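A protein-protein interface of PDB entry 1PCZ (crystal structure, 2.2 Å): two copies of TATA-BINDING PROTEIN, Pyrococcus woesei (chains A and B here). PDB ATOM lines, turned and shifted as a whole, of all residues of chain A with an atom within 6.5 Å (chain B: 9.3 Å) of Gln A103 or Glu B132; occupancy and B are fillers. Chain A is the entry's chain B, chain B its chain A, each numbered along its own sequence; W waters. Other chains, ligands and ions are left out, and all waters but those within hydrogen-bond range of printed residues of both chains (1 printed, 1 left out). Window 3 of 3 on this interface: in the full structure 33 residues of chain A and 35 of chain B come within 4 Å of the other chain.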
ATOM      1  N   ILE A  14      18.820  -2.217   7.721  1.00  0.00           N
ATOM      2  CA  ILE A  14      19.298  -2.694   6.431  1.00  0.00           C
ATOM      3  C   ILE A  14      19.446  -4.207   6.667  1.00  0.00           C
ATOM      4  O   ILE A  14      19.950  -4.654   7.717  1.00  0.00           O
ATOM      5  CB  ILE A  14      20.670  -2.112   6.023  1.00  0.00           C
ATOM      6  CG1 ILE A  14      20.681  -0.605   6.200  1.00  0.00           C
ATOM      7  CG2 ILE A  14      20.940  -2.417   4.570  1.00  0.00           C
ATOM      8  CD1 ILE A  14      21.929   0.069   5.705  1.00  0.00           C
ATOM      9  N   VAL A  15      18.855  -4.984   5.777  1.00  0.00           N
ATOM     10  CA  VAL A  15      18.944  -6.409   5.878  1.00  0.00           C
ATOM     11  C   VAL A  15      19.685  -6.837   4.642  1.00  0.00           C
ATOM     12  O   VAL A  15      19.457  -6.322   3.533  1.00  0.00           O
ATOM     13  CB  VAL A  15      17.582  -7.061   5.962  1.00  0.00           C
ATOM     14  CG1 VAL A  15      17.682  -8.553   5.727  1.00  0.00           C
ATOM     15  CG2 VAL A  15      17.019  -6.833   7.329  1.00  0.00           C
ATOM     16  N   ALA A  16      20.656  -7.714   4.835  1.00  0.00           N
ATOM     17  CA  ALA A  16      21.405  -8.176   3.692  1.00  0.00           C
ATOM     18  C   ALA A  16      21.365  -9.685   3.635  1.00  0.00           C
ATOM     19  O   ALA A  16      21.322 -10.373   4.662  1.00  0.00           O
ATOM     20  CB  ALA A  16      22.852  -7.684   3.773  1.00  0.00           C
ATOM     21  N   SER A  17      21.282 -10.191   2.422  1.00  0.00           N
ATOM     22  CA  SER A  17      21.317 -11.605   2.209  1.00  0.00           C
ATOM     23  C   SER A  17      22.805 -11.817   1.913  1.00  0.00           C
ATOM     24  O   SER A  17      23.447 -11.010   1.218  1.00  0.00           O
ATOM     25  CB  SER A  17      20.477 -11.964   0.992  1.00  0.00           C
ATOM     26  OG  SER A  17      20.935 -11.260  -0.159  1.00  0.00           O
ATOM     27  N   VAL A  18      23.382 -12.844   2.510  1.00  0.00           N
ATOM     28  CA  VAL A  18      24.781 -13.133   2.264  1.00  0.00           C
ATOM     29  C   VAL A  18      24.949 -14.598   1.979  1.00  0.00           C
ATOM     30  O   VAL A  18      24.257 -15.433   2.544  1.00  0.00           O
ATOM     31  CB  VAL A  18      25.648 -12.810   3.459  1.00  0.00           C
ATOM     32  CG1 VAL A  18      27.090 -13.057   3.110  1.00  0.00           C
ATOM     33  CG2 VAL A  18      25.428 -11.366   3.900  1.00  0.00           C
ATOM     34  N   ASP A 101      24.155  -8.980  -0.480  1.00  0.00           N
ATOM     35  CA  ASP A 101      23.170  -8.202  -1.212  1.00  0.00           C
ATOM     36  C   ASP A 101      22.204  -7.530  -0.277  1.00  0.00           C
ATOM     37  O   ASP A 101      21.541  -8.181   0.533  1.00  0.00           O
ATOM     38  CB  ASP A 101      22.381  -9.090  -2.156  1.00  0.00           C
ATOM     39  CG  ASP A 101      23.272  -9.858  -3.098  1.00  0.00           C
ATOM     40  OD1 ASP A 101      24.196  -9.260  -3.695  1.00  0.00           O
ATOM     41  OD2 ASP A 101      23.053 -11.072  -3.234  1.00  0.00           O
ATOM     42  N   VAL A 102      22.130  -6.215  -0.356  1.00  0.00           N
ATOM     43  CA  VAL A 102      21.184  -5.513   0.491  1.00  0.00           C
ATOM     44  C   VAL A 102      19.831  -5.995   0.022  1.00  0.00           C
ATOM     45  O   VAL A 102      19.560  -6.033  -1.176  1.00  0.00           O
ATOM     46  CB  VAL A 102      21.316  -3.970   0.373  1.00  0.00           C
ATOM     47  CG1 VAL A 102      20.032  -3.283   0.815  1.00  0.00           C
ATOM     48  CG2 VAL A 102      22.449  -3.508   1.281  1.00  0.00           C
ATOM     49  N   GLN A 103      19.063  -6.565   0.932  1.00  0.00           N
ATOM     50  CA  GLN A 103      17.745  -7.015   0.526  1.00  0.00           C
ATOM     51  C   GLN A 103      16.652  -6.019   0.873  1.00  0.00           C
ATOM     52  O   GLN A 103      15.671  -5.903   0.169  1.00  0.00           O
ATOM     53  CB  GLN A 103      17.442  -8.399   1.096  1.00  0.00           C
ATOM     54  CG  GLN A 103      18.465  -9.461   0.648  1.00  0.00           C
ATOM     55  CD  GLN A 103      18.464  -9.792  -0.863  1.00  0.00           C
ATOM     56  OE1 GLN A 103      18.418 -10.962  -1.238  1.00  0.00           O
ATOM     57  NE2 GLN A 103      18.575  -8.775  -1.719  1.00  0.00           N
ATOM     58  N   ASN A 104      16.887  -5.228   1.904  1.00  0.00           N
ATOM     59  CA  ASN A 104      15.887  -4.289   2.329  1.00  0.00           C
ATOM     60  C   ASN A 104      16.425  -3.244   3.259  1.00  0.00           C
ATOM     61  O   ASN A 104      17.258  -3.541   4.130  1.00  0.00           O
ATOM     62  CB  ASN A 104      14.771  -5.015   3.081  1.00  0.00           C
ATOM     63  CG  ASN A 104      13.586  -4.119   3.328  1.00  0.00           C
ATOM     64  OD1 ASN A 104      13.127  -3.470   2.414  1.00  0.00           O
ATOM     65  ND2 ASN A 104      13.092  -4.080   4.554  1.00  0.00           N
ATOM     66  N   MET A 105      15.894  -2.031   3.090  1.00  0.00           N
ATOM     67  CA  MET A 105      16.221  -0.897   3.942  1.00  0.00           C
ATOM     68  C   MET A 105      14.909  -0.352   4.408  1.00  0.00           C
ATOM     69  O   MET A 105      13.936  -0.361   3.683  1.00  0.00           O
ATOM     70  CB  MET A 105      16.986   0.169   3.199  1.00  0.00           C
ATOM     71  CG  MET A 105      18.332  -0.304   2.779  1.00  0.00           C
ATOM     72  SD  MET A 105      19.142   0.873   1.898  1.00  0.00           S
ATOM     73  CE  MET A 105      19.627   1.857   3.101  1.00  0.00           C
ATOM     74  N   ARG A 140       2.328   1.896  -1.924  1.00  0.00           N
ATOM     75  CA  ARG A 140       3.303   1.115  -2.620  1.00  0.00           C
ATOM     76  C   ARG A 140       3.745   1.844  -3.856  1.00  0.00           C
ATOM     77  O   ARG A 140       2.931   2.471  -4.542  1.00  0.00           O
ATOM     78  CB  ARG A 140       2.730  -0.247  -2.948  1.00  0.00           C
ATOM     79  CG  ARG A 140       2.360  -0.984  -1.717  1.00  0.00           C
ATOM     80  CD  ARG A 140       2.005  -2.373  -2.067  1.00  0.00           C
ATOM     81  NE  ARG A 140       1.420  -3.023  -0.912  1.00  0.00           N
ATOM     82  CZ  ARG A 140       2.131  -3.484   0.099  1.00  0.00           C
ATOM     83  NH1 ARG A 140       3.448  -3.373   0.043  1.00  0.00           N
ATOM     84  NH2 ARG A 140       1.529  -3.938   1.193  1.00  0.00           N
ATOM     85  N   LYS A 145      10.419  -0.204  -6.489  1.00  0.00           N
ATOM     86  CA  LYS A 145       9.492  -1.013  -5.700  1.00  0.00           C
ATOM     87  C   LYS A 145       9.828  -0.788  -4.228  1.00  0.00           C
ATOM     88  O   LYS A 145      10.944  -1.022  -3.777  1.00  0.00           O
ATOM     89  CB  LYS A 145       9.575  -2.487  -6.099  1.00  0.00           C
ATOM     90  CG  LYS A 145       9.175  -3.505  -5.032  1.00  0.00           C
ATOM     91  CD  LYS A 145       9.094  -4.954  -5.605  1.00  0.00           C
ATOM     92  CE  LYS A 145      10.261  -5.363  -6.590  1.00  0.00           C
ATOM     93  NZ  LYS A 145      11.660  -5.461  -6.027  1.00  0.00           N
ATOM     94  N   SER A 146       8.892  -0.167  -3.535  1.00  0.00           N
ATOM     95  CA  SER A 146       9.044   0.151  -2.132  1.00  0.00           C
ATOM     96  C   SER A 146       7.647   0.293  -1.569  1.00  0.00           C
ATOM     97  O   SER A 146       6.649   0.258  -2.312  1.00  0.00           O
ATOM     98  CB  SER A 146       9.820   1.459  -1.948  1.00  0.00           C
ATOM     99  OG  SER A 146      11.160   1.321  -2.424  1.00  0.00           O
ATOM    100  N   VAL A 147       7.571   0.411  -0.253  1.00  0.00           N
ATOM    101  CA  VAL A 147       6.302   0.544   0.416  1.00  0.00           C
ATOM    102  C   VAL A 147       6.491   1.587   1.475  1.00  0.00           C
ATOM    103  O   VAL A 147       7.483   1.558   2.206  1.00  0.00           O
ATOM    104  CB  VAL A 147       5.870  -0.794   1.070  1.00  0.00           C
ATOM    105  CG1 VAL A 147       6.956  -1.331   1.988  1.00  0.00           C
ATOM    106  CG2 VAL A 147       4.570  -0.627   1.807  1.00  0.00           C
ATOM    107  N   SER A 159       9.970   1.128   3.344  1.00  0.00           N
ATOM    108  CA  SER A 159      10.605  -0.158   3.360  1.00  0.00           C
ATOM    109  C   SER A 159      10.603  -0.654   1.922  1.00  0.00           C
ATOM    110  O   SER A 159       9.999  -0.038   1.049  1.00  0.00           O
ATOM    111  CB  SER A 159       9.810  -1.100   4.244  1.00  0.00           C
ATOM    112  OG  SER A 159      10.513  -2.301   4.504  1.00  0.00           O
ATOM    113  N   GLY A 160      11.336  -1.724   1.662  1.00  0.00           N
ATOM    114  CA  GLY A 160      11.373  -2.301   0.336  1.00  0.00           C
ATOM    115  C   GLY A 160      12.471  -1.761  -0.533  1.00  0.00           C
ATOM    116  O   GLY A 160      12.869  -2.411  -1.476  1.00  0.00           O
ATOM    117  N   ALA A 161      12.886  -0.528  -0.298  1.00  0.00           N
ATOM    118  CA  ALA A 161      13.954   0.034  -1.106  1.00  0.00           C
ATOM    119  C   ALA A 161      15.271  -0.602  -0.625  1.00  0.00           C
ATOM    120  O   ALA A 161      15.343  -1.174   0.484  1.00  0.00           O
ATOM    121  CB  ALA A 161      13.998   1.545  -0.982  1.00  0.00           C
ATOM    122  N   LYS A 162      16.294  -0.540  -1.473  1.00  0.00           N
ATOM    123  CA  LYS A 162      17.578  -1.129  -1.147  1.00  0.00           C
ATOM    124  C   LYS A 162      18.633  -0.064  -1.329  1.00  0.00           C
ATOM    125  O   LYS A 162      19.828  -0.336  -1.401  1.00  0.00           O
ATOM    126  CB  LYS A 162      17.836  -2.312  -2.075  1.00  0.00           C
ATOM    127  CG  LYS A 162      16.863  -3.429  -1.896  1.00  0.00           C
ATOM    128  CD  LYS A 162      16.964  -4.348  -3.057  1.00  0.00           C
ATOM    129  CE  LYS A 162      15.764  -5.266  -3.080  1.00  0.00           C
ATOM    130  NZ  LYS A 162      15.644  -6.007  -4.384  1.00  0.00           N
ATOM    131  N   ASP B 118      13.565  -9.005  12.709  1.00  0.00           N
ATOM    132  CA  ASP B 118      13.724 -10.346  12.187  1.00  0.00           C
ATOM    133  C   ASP B 118      13.781 -11.323  13.337  1.00  0.00           C
ATOM    134  O   ASP B 118      13.113 -12.343  13.322  1.00  0.00           O
ATOM    135  CB  ASP B 118      14.974 -10.422  11.357  1.00  0.00           C
ATOM    136  CG  ASP B 118      14.849  -9.633  10.097  1.00  0.00           C
ATOM    137  OD1 ASP B 118      14.924  -8.386  10.154  1.00  0.00           O
ATOM    138  OD2 ASP B 118      14.659 -10.257   9.048  1.00  0.00           O
ATOM    139  N   TYR B 129       5.552 -10.613   9.843  1.00  0.00           N
ATOM    140  CA  TYR B 129       6.679  -9.826   9.478  1.00  0.00           C
ATOM    141  C   TYR B 129       7.138 -10.152   8.093  1.00  0.00           C
ATOM    142  O   TYR B 129       7.599 -11.252   7.845  1.00  0.00           O
ATOM    143  CB  TYR B 129       7.811 -10.103  10.459  1.00  0.00           C
ATOM    144  CG  TYR B 129       9.066  -9.353  10.143  1.00  0.00           C
ATOM    145  CD1 TYR B 129       9.105  -7.955  10.230  1.00  0.00           C
ATOM    146  CD2 TYR B 129      10.239 -10.030   9.789  1.00  0.00           C
ATOM    147  CE1 TYR B 129      10.292  -7.251   9.983  1.00  0.00           C
ATOM    148  CE2 TYR B 129      11.424  -9.336   9.537  1.00  0.00           C
ATOM    149  CZ  TYR B 129      11.444  -7.953   9.643  1.00  0.00           C
ATOM    150  OH  TYR B 129      12.615  -7.268   9.457  1.00  0.00           O
ATOM    151  N   GLU B 130       6.915  -9.216   7.184  1.00  0.00           N
ATOM    152  CA  GLU B 130       7.381  -9.314   5.822  1.00  0.00           C
ATOM    153  C   GLU B 130       7.648  -7.873   5.424  1.00  0.00           C
ATOM    154  O   GLU B 130       6.910  -7.275   4.653  1.00  0.00           O
ATOM    155  CB  GLU B 130       6.398 -10.042   4.909  1.00  0.00           C
ATOM    156  CG  GLU B 130       5.081  -9.410   4.654  1.00  0.00           C
ATOM    157  CD  GLU B 130       4.311 -10.201   3.619  1.00  0.00           C
ATOM    158  OE1 GLU B 130       4.779 -10.285   2.454  1.00  0.00           O
ATOM    159  OE2 GLU B 130       3.256 -10.767   3.988  1.00  0.00           O
ATOM    160  N   PRO B 131       8.791  -7.333   5.900  1.00  0.00           N
ATOM    161  CA  PRO B 131       9.286  -5.965   5.702  1.00  0.00           C
ATOM    162  C   PRO B 131       9.249  -5.398   4.300  1.00  0.00           C
ATOM    163  O   PRO B 131       8.990  -4.211   4.113  1.00  0.00           O
ATOM    164  CB  PRO B 131      10.697  -6.024   6.283  1.00  0.00           C
ATOM    165  CG  PRO B 131      11.093  -7.428   6.065  1.00  0.00           C
ATOM    166  CD  PRO B 131       9.863  -8.186   6.447  1.00  0.00           C
ATOM    167  N   GLU B 132       9.477  -6.238   3.310  1.00  0.00           N
ATOM    168  CA  GLU B 132       9.466  -5.763   1.934  1.00  0.00           C
ATOM    169  C   GLU B 132       8.064  -5.241   1.607  1.00  0.00           C
ATOM    170  O   GLU B 132       7.901  -4.172   1.002  1.00  0.00           O
ATOM    171  CB  GLU B 132       9.798  -6.918   0.981  1.00  0.00           C
ATOM    172  CG  GLU B 132      10.857  -7.898   1.490  1.00  0.00           C
ATOM    173  CD  GLU B 132      12.208  -7.248   1.750  1.00  0.00           C
ATOM    174  OE1 GLU B 132      12.399  -6.081   1.330  1.00  0.00           O
ATOM    175  OE2 GLU B 132      13.070  -7.915   2.374  1.00  0.00           O
ATOM    176  N   GLN B 133       7.080  -6.042   2.017  1.00  0.00           N
ATOM    177  CA  GLN B 133       5.665  -5.797   1.809  1.00  0.00           C
ATOM    178  C   GLN B 133       5.066  -4.787   2.789  1.00  0.00           C
ATOM    179  O   GLN B 133       4.275  -3.917   2.427  1.00  0.00           O
ATOM    180  CB  GLN B 133       4.936  -7.132   1.940  1.00  0.00           C
ATOM    181  CG  GLN B 133       3.431  -7.080   1.763  1.00  0.00           C
ATOM    182  CD  GLN B 133       2.982  -7.148   0.295  1.00  0.00           C
ATOM    183  OE1 GLN B 133       3.633  -6.602  -0.612  1.00  0.00           O
ATOM    184  NE2 GLN B 133       1.851  -7.816   0.060  1.00  0.00           N
ATOM    185  N   PHE B 134       5.470  -4.868   4.038  1.00  0.00           N
ATOM    186  CA  PHE B 134       4.912  -3.984   5.024  1.00  0.00           C
ATOM    187  C   PHE B 134       5.958  -3.796   6.082  1.00  0.00           C
ATOM    188  O   PHE B 134       6.455  -4.768   6.631  1.00  0.00           O
ATOM    189  CB  PHE B 134       3.667  -4.659   5.628  1.00  0.00           C
ATOM    190  CG  PHE B 134       2.891  -3.784   6.568  1.00  0.00           C
ATOM    191  CD1 PHE B 134       3.196  -3.748   7.921  1.00  0.00           C
ATOM    192  CD2 PHE B 134       1.840  -2.998   6.100  1.00  0.00           C
ATOM    193  CE1 PHE B 134       2.478  -2.953   8.780  1.00  0.00           C
ATOM    194  CE2 PHE B 134       1.112  -2.194   6.972  1.00  0.00           C
ATOM    195  CZ  PHE B 134       1.432  -2.175   8.310  1.00  0.00           C
ATOM    196  N   PRO B 135       6.312  -2.543   6.388  1.00  0.00           N
ATOM    197  CA  PRO B 135       7.327  -2.362   7.423  1.00  0.00           C
ATOM    198  C   PRO B 135       6.817  -2.703   8.808  1.00  0.00           C
ATOM    199  O   PRO B 135       5.626  -2.587   9.092  1.00  0.00           O
ATOM    200  CB  PRO B 135       7.681  -0.874   7.306  1.00  0.00           C
ATOM    201  CG  PRO B 135       6.445  -0.257   6.778  1.00  0.00           C
ATOM    202  CD  PRO B 135       5.984  -1.254   5.743  1.00  0.00           C
ATOM    203  N   GLY B 136       7.725  -3.194   9.643  1.00  0.00           N
ATOM    204  CA  GLY B 136       7.387  -3.493  11.011  1.00  0.00           C
ATOM    205  C   GLY B 136       6.873  -4.886  11.192  1.00  0.00           C
ATOM    206  O   GLY B 136       6.671  -5.615  10.227  1.00  0.00           O
HETATM  207  O   HOH W   1      14.194  -7.250   5.441  1.00  0.00           O
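OG of Ser A159 sits at hydrogen-bond distance from O of Pro B131 (2.5 Å). The side-chain amide oxygen (OD1) of Asn A104 lies close to the side-chain carboxylate (OE1) of Glu B132. The guanidinium group (NH1) of Arg A140 is in hydrogen-bond range of the backbone carbonyl oxygen (O) of Gln B133 (2.6 Å). The side-chain carboxylate (OE1) of Glu B132 lies close to the backbone carbonyl oxygen (O) of Gln A103.
The side-chain carboxylate (OD1) of Asp B118 lies within hydrogen-bond range of the side-chain hydroxyl (OH) of Tyr B129. The backbone carbonyl oxygen of Val A15 is in hydrogen-bond range of the backbone NH of Gln A103 (2.6 Å). The side-chain hydroxyl of Ser A17 sits at hydrogen-bond distance from the side-chain amide oxygen of Gln A103 (2.8 Å). ND2 of Asn A104 is in hydrogen-bond range of OG of Ser A159 (3.1 Å). The backbone NH (N) of Gly A160 lies within hydrogen-bond range of the side-chain amide oxygen (OD1) of Asn A104 (2.6 Å). O of Val A147 lies within hydrogen-bond range of N of Ser A159 (2.8 Å).
Among the printed residues, merely in contact across the chains: Val A147 with Glu B132 (3.2 Å), Val A147 with Gln B133 (3.4 Å), Asn A104 with Pro B131 (3.5 Å), Ser A159 with Pro B135 (3.7 Å), Val A15 with Asp B118 (3.8 Å), Val A147 with Pro B135 (3.9 Å) and Gly A160 with Glu B132 (3.9999 Å).
Of the printed residues of chain A, Glu B132 touches Gln A103, Asn A104, Val A147 and Gly A160. No residue of chain B comes within 4 Å of Ala A16. Asn A104 touches two residues of chain B. Printed residues of chain A within 4 Å of Pro B131: Asn A104 and Ser A159. Of the printed residues of chain B, Ser A159 touches Pro B131 (2.5 Å) and Pro B135 (3.7 Å). Of the printed residues of chain B, Val A15 touches Asp B118 (3.8 Å). Printed residues of chain A within 4 Å of Gln B133: Arg A140 and Val A147. Of the printed residues of chain B, Gly A160 touches Glu B132 (3.9999 Å).
Of the 9 printed residues of chain B, 5 touch a printed residue of chain A.
No position is printed for both chains.
Water W1 bridges the side-chain carboxylate (OE2) of Glu B132 and the side-chain amide nitrogen (ND2) of Asn A104.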
